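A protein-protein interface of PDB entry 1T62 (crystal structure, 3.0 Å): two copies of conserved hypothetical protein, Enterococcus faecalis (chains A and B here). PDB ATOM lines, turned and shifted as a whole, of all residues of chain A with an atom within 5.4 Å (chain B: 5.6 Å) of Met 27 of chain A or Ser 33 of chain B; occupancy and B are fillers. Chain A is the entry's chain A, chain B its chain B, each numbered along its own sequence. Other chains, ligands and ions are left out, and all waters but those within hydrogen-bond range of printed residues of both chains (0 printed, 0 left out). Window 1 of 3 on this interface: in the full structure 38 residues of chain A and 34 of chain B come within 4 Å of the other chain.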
ATOM      1  N   VAL A  25      18.058  36.927 -21.898  1.00  0.00           N
ATOM      2  CA  VAL A  25      17.918  36.203 -23.149  1.00  0.00           C
ATOM      3  C   VAL A  25      17.419  34.789 -22.880  1.00  0.00           C
ATOM      4  O   VAL A  25      17.978  34.068 -22.047  1.00  0.00           O
ATOM      5  CB  VAL A  25      19.244  36.155 -23.932  1.00  0.00           C
ATOM      6  CG1 VAL A  25      19.729  37.573 -24.203  1.00  0.00           C
ATOM      7  CG2 VAL A  25      20.271  35.356 -23.174  1.00  0.00           C
ATOM      8  N   TRP A  26      16.360  34.395 -23.581  1.00  0.00           N
ATOM      9  CA  TRP A  26      15.798  33.075 -23.384  1.00  0.00           C
ATOM     10  C   TRP A  26      14.827  32.618 -24.468  1.00  0.00           C
ATOM     11  O   TRP A  26      14.412  33.392 -25.328  1.00  0.00           O
ATOM     12  CB  TRP A  26      15.097  33.005 -22.024  1.00  0.00           C
ATOM     13  CG  TRP A  26      14.255  34.194 -21.734  1.00  0.00           C
ATOM     14  CD1 TRP A  26      14.661  35.354 -21.148  1.00  0.00           C
ATOM     15  CD2 TRP A  26      12.872  34.381 -22.075  1.00  0.00           C
ATOM     16  NE1 TRP A  26      13.625  36.255 -21.102  1.00  0.00           N
ATOM     17  CE2 TRP A  26      12.514  35.686 -21.664  1.00  0.00           C
ATOM     18  CE3 TRP A  26      11.902  33.576 -22.691  1.00  0.00           C
ATOM     19  CZ2 TRP A  26      11.228  36.207 -21.849  1.00  0.00           C
ATOM     20  CZ3 TRP A  26      10.620  34.094 -22.877  1.00  0.00           C
ATOM     21  CH2 TRP A  26      10.297  35.401 -22.456  1.00  0.00           C
ATOM     22  N   MET A  27      14.479  31.333 -24.398  1.00  0.00           N
ATOM     23  CA  MET A  27      13.550  30.707 -25.322  1.00  0.00           C
ATOM     24  C   MET A  27      12.356  30.215 -24.501  1.00  0.00           C
ATOM     25  O   MET A  27      12.490  29.889 -23.322  1.00  0.00           O
ATOM     26  CB  MET A  27      14.216  29.524 -26.039  1.00  0.00           C
ATOM     27  CG  MET A  27      14.469  28.309 -25.160  1.00  0.00           C
ATOM     28  SD  MET A  27      15.143  26.867 -26.042  1.00  0.00           S
ATOM     29  CE  MET A  27      16.836  26.808 -25.447  1.00  0.00           C
ATOM     30  N   PHE A  28      11.186  30.189 -25.129  1.00  0.00           N
ATOM     31  CA  PHE A  28       9.972  29.739 -24.474  1.00  0.00           C
ATOM     32  C   PHE A  28      10.013  28.228 -24.437  1.00  0.00           C
ATOM     33  O   PHE A  28      10.709  27.614 -25.237  1.00  0.00           O
ATOM     34  CB  PHE A  28       8.756  30.167 -25.285  1.00  0.00           C
ATOM     35  CG  PHE A  28       8.550  31.647 -25.339  1.00  0.00           C
ATOM     36  CD1 PHE A  28       7.722  32.282 -24.414  1.00  0.00           C
ATOM     37  CD2 PHE A  28       9.182  32.414 -26.313  1.00  0.00           C
ATOM     38  CE1 PHE A  28       7.527  33.661 -24.458  1.00  0.00           C
ATOM     39  CE2 PHE A  28       8.996  33.792 -26.368  1.00  0.00           C
ATOM     40  CZ  PHE A  28       8.166  34.418 -25.437  1.00  0.00           C
ATOM     41  N   GLY A  29       9.289  27.620 -23.507  1.00  0.00           N
ATOM     42  CA  GLY A  29       9.255  26.173 -23.477  1.00  0.00           C
ATOM     43  C   GLY A  29       9.860  25.406 -22.325  1.00  0.00           C
ATOM     44  O   GLY A  29      10.506  25.960 -21.439  1.00  0.00           O
ATOM     45  N   GLY A  31      12.209  23.493 -22.530  1.00  0.00           N
ATOM     46  CA  GLY A  31      13.652  23.560 -22.646  1.00  0.00           C
ATOM     47  C   GLY A  31      14.035  22.825 -23.908  1.00  0.00           C
ATOM     48  O   GLY A  31      15.137  22.983 -24.434  1.00  0.00           O
ATOM     49  N   SER A  32      13.107  22.004 -24.388  1.00  0.00           N
ATOM     50  CA  SER A  32      13.318  21.242 -25.606  1.00  0.00           C
ATOM     51  C   SER A  32      13.368  22.232 -26.754  1.00  0.00           C
ATOM     52  O   SER A  32      12.723  23.281 -26.709  1.00  0.00           O
ATOM     53  CB  SER A  32      12.164  20.267 -25.838  1.00  0.00           C
ATOM     54  OG  SER A  32      10.954  20.961 -26.095  1.00  0.00           O
ATOM     55  N   SER A  33      14.132  21.900 -27.783  1.00  0.00           N
ATOM     56  CA  SER A  33      14.245  22.778 -28.931  1.00  0.00           C
ATOM     57  C   SER A  33      12.922  22.871 -29.690  1.00  0.00           C
ATOM     58  O   SER A  33      12.603  23.896 -30.293  1.00  0.00           O
ATOM     59  CB  SER A  33      15.346  22.272 -29.857  1.00  0.00           C
ATOM     60  OG  SER A  33      15.149  20.904 -30.143  1.00  0.00           O
ATOM     61  N   GLY A  36      10.646  25.290 -28.056  1.00  0.00           N
ATOM     62  CA  GLY A  36      11.263  26.593 -28.233  1.00  0.00           C
ATOM     63  C   GLY A  36      11.027  27.160 -29.621  1.00  0.00           C
ATOM     64  O   GLY A  36      10.737  28.345 -29.795  1.00  0.00           O
ATOM     65  N   ILE A  74      14.490  37.108 -27.296  1.00  0.00           N
ATOM     66  CA  ILE A  74      13.990  35.759 -27.552  1.00  0.00           C
ATOM     67  C   ILE A  74      14.851  34.978 -28.527  1.00  0.00           C
ATOM     68  O   ILE A  74      15.255  35.502 -29.563  1.00  0.00           O
ATOM     69  CB  ILE A  74      12.551  35.802 -28.097  1.00  0.00           C
ATOM     70  CG1 ILE A  74      11.675  36.635 -27.159  1.00  0.00           C
ATOM     71  CG2 ILE A  74      12.004  34.393 -28.261  1.00  0.00           C
ATOM     72  CD1 ILE A  74      11.827  36.278 -25.699  1.00  0.00           C
ATOM     73  N   LEU A  75      15.112  33.720 -28.172  1.00  0.00           N
ATOM     74  CA  LEU A  75      15.931  32.795 -28.954  1.00  0.00           C
ATOM     75  C   LEU A  75      15.066  31.605 -29.324  1.00  0.00           C
ATOM     76  O   LEU A  75      14.040  31.374 -28.690  1.00  0.00           O
ATOM     77  CB  LEU A  75      17.106  32.287 -28.112  1.00  0.00           C
ATOM     78  CG  LEU A  75      18.030  33.263 -27.375  1.00  0.00           C
ATOM     79  CD1 LEU A  75      18.950  32.457 -26.473  1.00  0.00           C
ATOM     80  CD2 LEU A  75      18.844  34.114 -28.369  1.00  0.00           C
ATOM     81  N   ASP A  76      15.476  30.843 -30.334  1.00  0.00           N
ATOM     82  CA  ASP A  76      14.708  29.666 -30.733  1.00  0.00           C
ATOM     83  C   ASP A  76      15.201  28.426 -30.001  1.00  0.00           C
ATOM     84  O   ASP A  76      16.110  28.499 -29.169  1.00  0.00           O
ATOM     85  CB  ASP A  76      14.781  29.425 -32.249  1.00  0.00           C
ATOM     86  CG  ASP A  76      16.195  29.213 -32.747  1.00  0.00           C
ATOM     87  OD1 ASP A  76      17.063  28.823 -31.941  1.00  0.00           O
ATOM     88  OD2 ASP A  76      16.440  29.426 -33.954  1.00  0.00           O
ATOM     89  N   GLY A  77      14.596  27.286 -30.316  1.00  0.00           N
ATOM     90  CA  GLY A  77      14.978  26.045 -29.680  1.00  0.00           C
ATOM     91  C   GLY A  77      16.442  25.721 -29.878  1.00  0.00           C
ATOM     92  O   GLY A  77      17.006  24.925 -29.128  1.00  0.00           O
ATOM     93  N   GLN A  78      17.053  26.333 -30.890  1.00  0.00           N
ATOM     94  CA  GLN A  78      18.471  26.125 -31.208  1.00  0.00           C
ATOM     95  C   GLN A  78      19.315  27.236 -30.609  1.00  0.00           C
ATOM     96  O   GLN A  78      20.503  27.350 -30.902  1.00  0.00           O
ATOM     97  CB  GLN A  78      18.690  26.097 -32.724  1.00  0.00           C
ATOM     98  CG  GLN A  78      18.995  24.714 -33.287  1.00  0.00           C
ATOM     99  CD  GLN A  78      17.836  23.748 -33.134  1.00  0.00           C
ATOM    100  OE1 GLN A  78      16.751  23.972 -33.675  1.00  0.00           O
ATOM    101  NE2 GLN A  78      18.062  22.663 -32.394  1.00  0.00           N
ATOM    102  N   SER A  79      18.678  28.056 -29.779  1.00  0.00           N
ATOM    103  CA  SER A  79      19.329  29.172 -29.107  1.00  0.00           C
ATOM    104  C   SER A  79      19.798  30.322 -29.984  1.00  0.00           C
ATOM    105  O   SER A  79      20.825  30.931 -29.695  1.00  0.00           O
ATOM    106  CB  SER A  79      20.501  28.669 -28.275  1.00  0.00           C
ATOM    107  OG  SER A  79      20.023  27.925 -27.169  1.00  0.00           O
ATOM    108  N   MET B  27      28.306  27.447 -25.625  1.00  0.00           N
ATOM    109  CA  MET B  27      27.781  26.295 -24.911  1.00  0.00           C
ATOM    110  C   MET B  27      28.136  25.093 -25.774  1.00  0.00           C
ATOM    111  O   MET B  27      28.414  25.256 -26.962  1.00  0.00           O
ATOM    112  CB  MET B  27      26.264  26.403 -24.698  1.00  0.00           C
ATOM    113  CG  MET B  27      25.414  26.222 -25.926  1.00  0.00           C
ATOM    114  SD  MET B  27      23.649  26.420 -25.548  1.00  0.00           S
ATOM    115  CE  MET B  27      23.113  24.779 -25.504  1.00  0.00           C
ATOM    116  N   GLY B  31      23.302  23.995 -29.700  1.00  0.00           N
ATOM    117  CA  GLY B  31      22.477  25.085 -29.218  1.00  0.00           C
ATOM    118  C   GLY B  31      21.240  24.572 -28.507  1.00  0.00           C
ATOM    119  O   GLY B  31      20.530  25.336 -27.857  1.00  0.00           O
ATOM    120  N   SER B  32      20.964  23.281 -28.644  1.00  0.00           N
ATOM    121  CA  SER B  32      19.820  22.693 -27.967  1.00  0.00           C
ATOM    122  C   SER B  32      20.086  22.816 -26.470  1.00  0.00           C
ATOM    123  O   SER B  32      21.197  22.554 -25.994  1.00  0.00           O
ATOM    124  CB  SER B  32      19.682  21.214 -28.320  1.00  0.00           C
ATOM    125  OG  SER B  32      19.666  21.029 -29.718  1.00  0.00           O
ATOM    126  N   SER B  33      19.066  23.219 -25.725  1.00  0.00           N
ATOM    127  CA  SER B  33      19.214  23.352 -24.290  1.00  0.00           C
ATOM    128  C   SER B  33      19.662  22.002 -23.724  1.00  0.00           C
ATOM    129  O   SER B  33      20.684  21.911 -23.046  1.00  0.00           O
ATOM    130  CB  SER B  33      17.888  23.770 -23.671  1.00  0.00           C
ATOM    131  OG  SER B  33      18.084  24.180 -22.336  1.00  0.00           O
ATOM    132  N   GLU B  34      18.901  20.953 -24.018  1.00  0.00           N
ATOM    133  CA  GLU B  34      19.220  19.613 -23.537  1.00  0.00           C
ATOM    134  C   GLU B  34      20.699  19.281 -23.710  1.00  0.00           C
ATOM    135  O   GLU B  34      21.417  19.065 -22.733  1.00  0.00           O
ATOM    136  CB  GLU B  34      18.369  18.565 -24.269  1.00  0.00           C
ATOM    137  CG  GLU B  34      17.248  17.938 -23.418  1.00  0.00           C
ATOM    138  CD  GLU B  34      15.965  18.772 -23.350  1.00  0.00           C
ATOM    139  OE1 GLU B  34      15.245  18.862 -24.371  1.00  0.00           O
ATOM    140  OE2 GLU B  34      15.675  19.334 -22.270  1.00  0.00           O
ATOM    141  N   MET B  35      21.154  19.244 -24.958  1.00  0.00           N
ATOM    142  CA  MET B  35      22.548  18.931 -25.238  1.00  0.00           C
ATOM    143  C   MET B  35      23.465  19.912 -24.536  1.00  0.00           C
ATOM    144  O   MET B  35      24.538  19.541 -24.074  1.00  0.00           O
ATOM    145  CB  MET B  35      22.804  18.975 -26.740  1.00  0.00           C
ATOM    146  CG  MET B  35      24.211  18.592 -27.138  1.00  0.00           C
ATOM    147  SD  MET B  35      24.371  18.196 -28.912  1.00  0.00           S
ATOM    148  CE  MET B  35      23.929  16.419 -28.861  1.00  0.00           C
ATOM    149  N   GLY B  36      23.025  21.164 -24.452  1.00  0.00           N
ATOM    150  CA  GLY B  36      23.816  22.200 -23.809  1.00  0.00           C
ATOM    151  C   GLY B  36      24.101  21.934 -22.349  1.00  0.00           C
ATOM    152  O   GLY B  36      25.207  22.193 -21.858  1.00  0.00           O
ATOM    153  N   ASN B  37      23.094  21.415 -21.654  1.00  0.00           N
ATOM    154  CA  ASN B  37      23.212  21.092 -20.234  1.00  0.00           C
ATOM    155  C   ASN B  37      23.878  19.722 -20.041  1.00  0.00           C
ATOM    156  O   ASN B  37      24.784  19.572 -19.215  1.00  0.00           O
ATOM    157  CB  ASN B  37      21.820  21.110 -19.592  1.00  0.00           C
ATOM    158  CG  ASN B  37      21.230  22.515 -19.513  1.00  0.00           C
ATOM    159  OD1 ASN B  37      20.022  22.709 -19.653  1.00  0.00           O
ATOM    160  ND2 ASN B  37      22.089  23.502 -19.277  1.00  0.00           N
ATOM    161  N   ARG B  38      23.430  18.734 -20.815  1.00  0.00           N
ATOM    162  CA  ARG B  38      23.977  17.384 -20.752  1.00  0.00           C
ATOM    163  C   ARG B  38      25.489  17.445 -20.786  1.00  0.00           C
ATOM    164  O   ARG B  38      26.154  16.919 -19.901  1.00  0.00           O
ATOM    165  CB  ARG B  38      23.481  16.557 -21.936  1.00  0.00           C
ATOM    166  CG  ARG B  38      23.853  15.085 -21.884  1.00  0.00           C
ATOM    167  CD  ARG B  38      23.103  14.294 -22.950  1.00  0.00           C
ATOM    168  NE  ARG B  38      23.565  14.546 -24.319  1.00  0.00           N
ATOM    169  CZ  ARG B  38      24.700  14.071 -24.833  1.00  0.00           C
ATOM    170  NH1 ARG B  38      25.026  14.353 -26.092  1.00  0.00           N
ATOM    171  NH2 ARG B  38      25.511  13.311 -24.096  1.00  0.00           N
ATOM    172  N   ASP B  76      25.695  27.040 -20.185  1.00  0.00           N
ATOM    173  CA  ASP B  76      24.865  25.841 -20.090  1.00  0.00           C
ATOM    174  C   ASP B  76      23.714  25.955 -21.097  1.00  0.00           C
ATOM    175  O   ASP B  76      23.675  26.900 -21.892  1.00  0.00           O
ATOM    176  CB  ASP B  76      24.342  25.644 -18.657  1.00  0.00           C
ATOM    177  CG  ASP B  76      23.398  26.755 -18.195  1.00  0.00           C
ATOM    178  OD1 ASP B  76      23.350  27.837 -18.819  1.00  0.00           O
ATOM    179  OD2 ASP B  76      22.705  26.543 -17.179  1.00  0.00           O
ATOM    180  N   GLY B  77      22.800  24.993 -21.079  1.00  0.00           N
ATOM    181  CA  GLY B  77      21.682  25.011 -22.007  1.00  0.00           C
ATOM    182  C   GLY B  77      20.888  26.304 -22.068  1.00  0.00           C
ATOM    183  O   GLY B  77      20.386  26.673 -23.132  1.00  0.00           O
ATOM    184  N   GLN B  78      20.769  26.993 -20.932  1.00  0.00           N
ATOM    185  CA  GLN B  78      20.032  28.252 -20.857  1.00  0.00           C
ATOM    186  C   GLN B  78      20.915  29.455 -21.110  1.00  0.00           C
ATOM    187  O   GLN B  78      20.650  30.536 -20.593  1.00  0.00           O
ATOM    188  CB  GLN B  78      19.380  28.425 -19.490  1.00  0.00           C
ATOM    189  CG  GLN B  78      18.274  27.459 -19.215  1.00  0.00           C
ATOM    190  CD  GLN B  78      18.783  26.105 -18.818  1.00  0.00           C
ATOM    191  OE1 GLN B  78      18.031  25.137 -18.785  1.00  0.00           O
ATOM    192  NE2 GLN B  78      20.070  26.027 -18.499  1.00  0.00           N
ATOM    193  N   HIS B 165       9.344  29.862 -19.282  1.00  0.00           N
ATOM    194  CA  HIS B 165       8.267  30.719 -19.754  1.00  0.00           C
ATOM    195  C   HIS B 165       7.410  29.911 -20.698  1.00  0.00           C
ATOM    196  O   HIS B 165       7.927  29.293 -21.624  1.00  0.00           O
ATOM    197  CB  HIS B 165       8.803  31.926 -20.518  1.00  0.00           C
ATOM    198  CG  HIS B 165       9.671  32.824 -19.704  1.00  0.00           C
ATOM    199  ND1 HIS B 165      10.991  32.537 -19.434  1.00  0.00           N
ATOM    200  CD2 HIS B 165       9.410  34.008 -19.103  1.00  0.00           C
ATOM    201  CE1 HIS B 165      11.508  33.508 -18.702  1.00  0.00           C
ATOM    202  NE2 HIS B 165      10.569  34.413 -18.487  1.00  0.00           N
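N of Gly 29 of chain A sits at hydrogen-bond distance from O of His 165 of chain B, 2.9 Å away.
The backbone carbonyl oxygen of Gly 31 of chain B lies within hydrogen-bond range of the side-chain hydroxyl of Ser 79 of chain A, 2.7 Å away.
The backbone NH (N) of Leu 75 of chain A sits at hydrogen-bond distance from the backbone carbonyl oxygen (O) of Trp 26 of chain A, 2.9 Å away.
The side-chain carboxylate (OD1) of Asp 76 of chain A is in hydrogen-bond range of the backbone NH (N) of Gln 78 of chain A, at 2.7 Å.
OD1 of Asp 76 of chain A sits at hydrogen-bond distance from N of Ser 79 of chain A.
OG of Ser 33 of chain B sits at hydrogen-bond distance from O of Gly 77 of chain B (3.5 Å).
Among the printed residues, merely in contact across the chains: Trp 26 of chain A with His 165 of chain B, Met 27 of chain A with Ser 33 of chain B, Phe 28 of chain A with His 165 of chain B, Gly 31 of chain A with Ser 33 of chain B, Ser 32 of chain A with Glu 34 of chain B, Gly 77 of chain A with Gly 31 of chain B, Gly 77 of chain A with Ser 32 of chain B, Gln 78 of chain A with Gly 31 of chain B and Gln 78 of chain A with Ser 32 of chain B.
Of chain B, only Ser 33 (3.7 Å) comes within 4 Å of Met 27 of chain A.
Ser 33 of chain B touches just these residues of chain A: Met 27 and Gly 31.
Of the printed residues of chain B, Gln 78 of chain A touches Gly 31 and Ser 32.
Of the printed residues of chain B, Trp 26 of chain A touches His 165 (3.5 Å).
Printed residues of chain A within 4 Å of Glu 34 of chain B: Ser 32.
The nearest residue of chain B that does not touch Met 27 of chain A is Gly 77 of chain B (4.2 Å).
The nearest residue of chain A that does not touch Ser 33 of chain B is Gly 77 of chain A (4.3 Å).
Of the 13 printed residues of chain B, 5 touch a printed residue of chain A.
Hydrophobic or aromatic side chains of chain B within 4 Å of the printed part of chain A: His 165.
Of the 15 printed residues of chain A, 9 touch a printed residue of chain B.
Hydrophobic or aromatic side chains of chain A within 4 Å of the printed part of chain B: Trp 26, Met 27 and Phe 28.
Among the printed residues, 11 pairs touch across the chains.
Among the printed residues, no Asp or Glu carboxylate lies within 4 Å of a Lys or Arg side-chain nitrogen of the other chain.
Met 27 of chain A touches Ser 33 of chain B, but with the chains exchanged Ser 33 of chain A does not touch Met 27 of chain B (9.2 Å).
Gly 31 of chain A touches Ser 33 of chain B, but with the chains exchanged Ser 33 of chain A does not touch Gly 31 of chain B (6.3 Å).
Gly 77 of chain A touches Gly 31 of chain B, but with the chains exchanged Gly 31 of chain A does not touch Gly 77 of chain B (6.5 Å).
Gln 78 of chain A touches Gly 31 of chain B, but with the chains exchanged Gly 31 of chain A does not touch Gln 78 of chain B (6.0 Å).
Of the 11 pairs that touch across the chains among the printed residues, none has its exchanged pair printed and touching as well.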
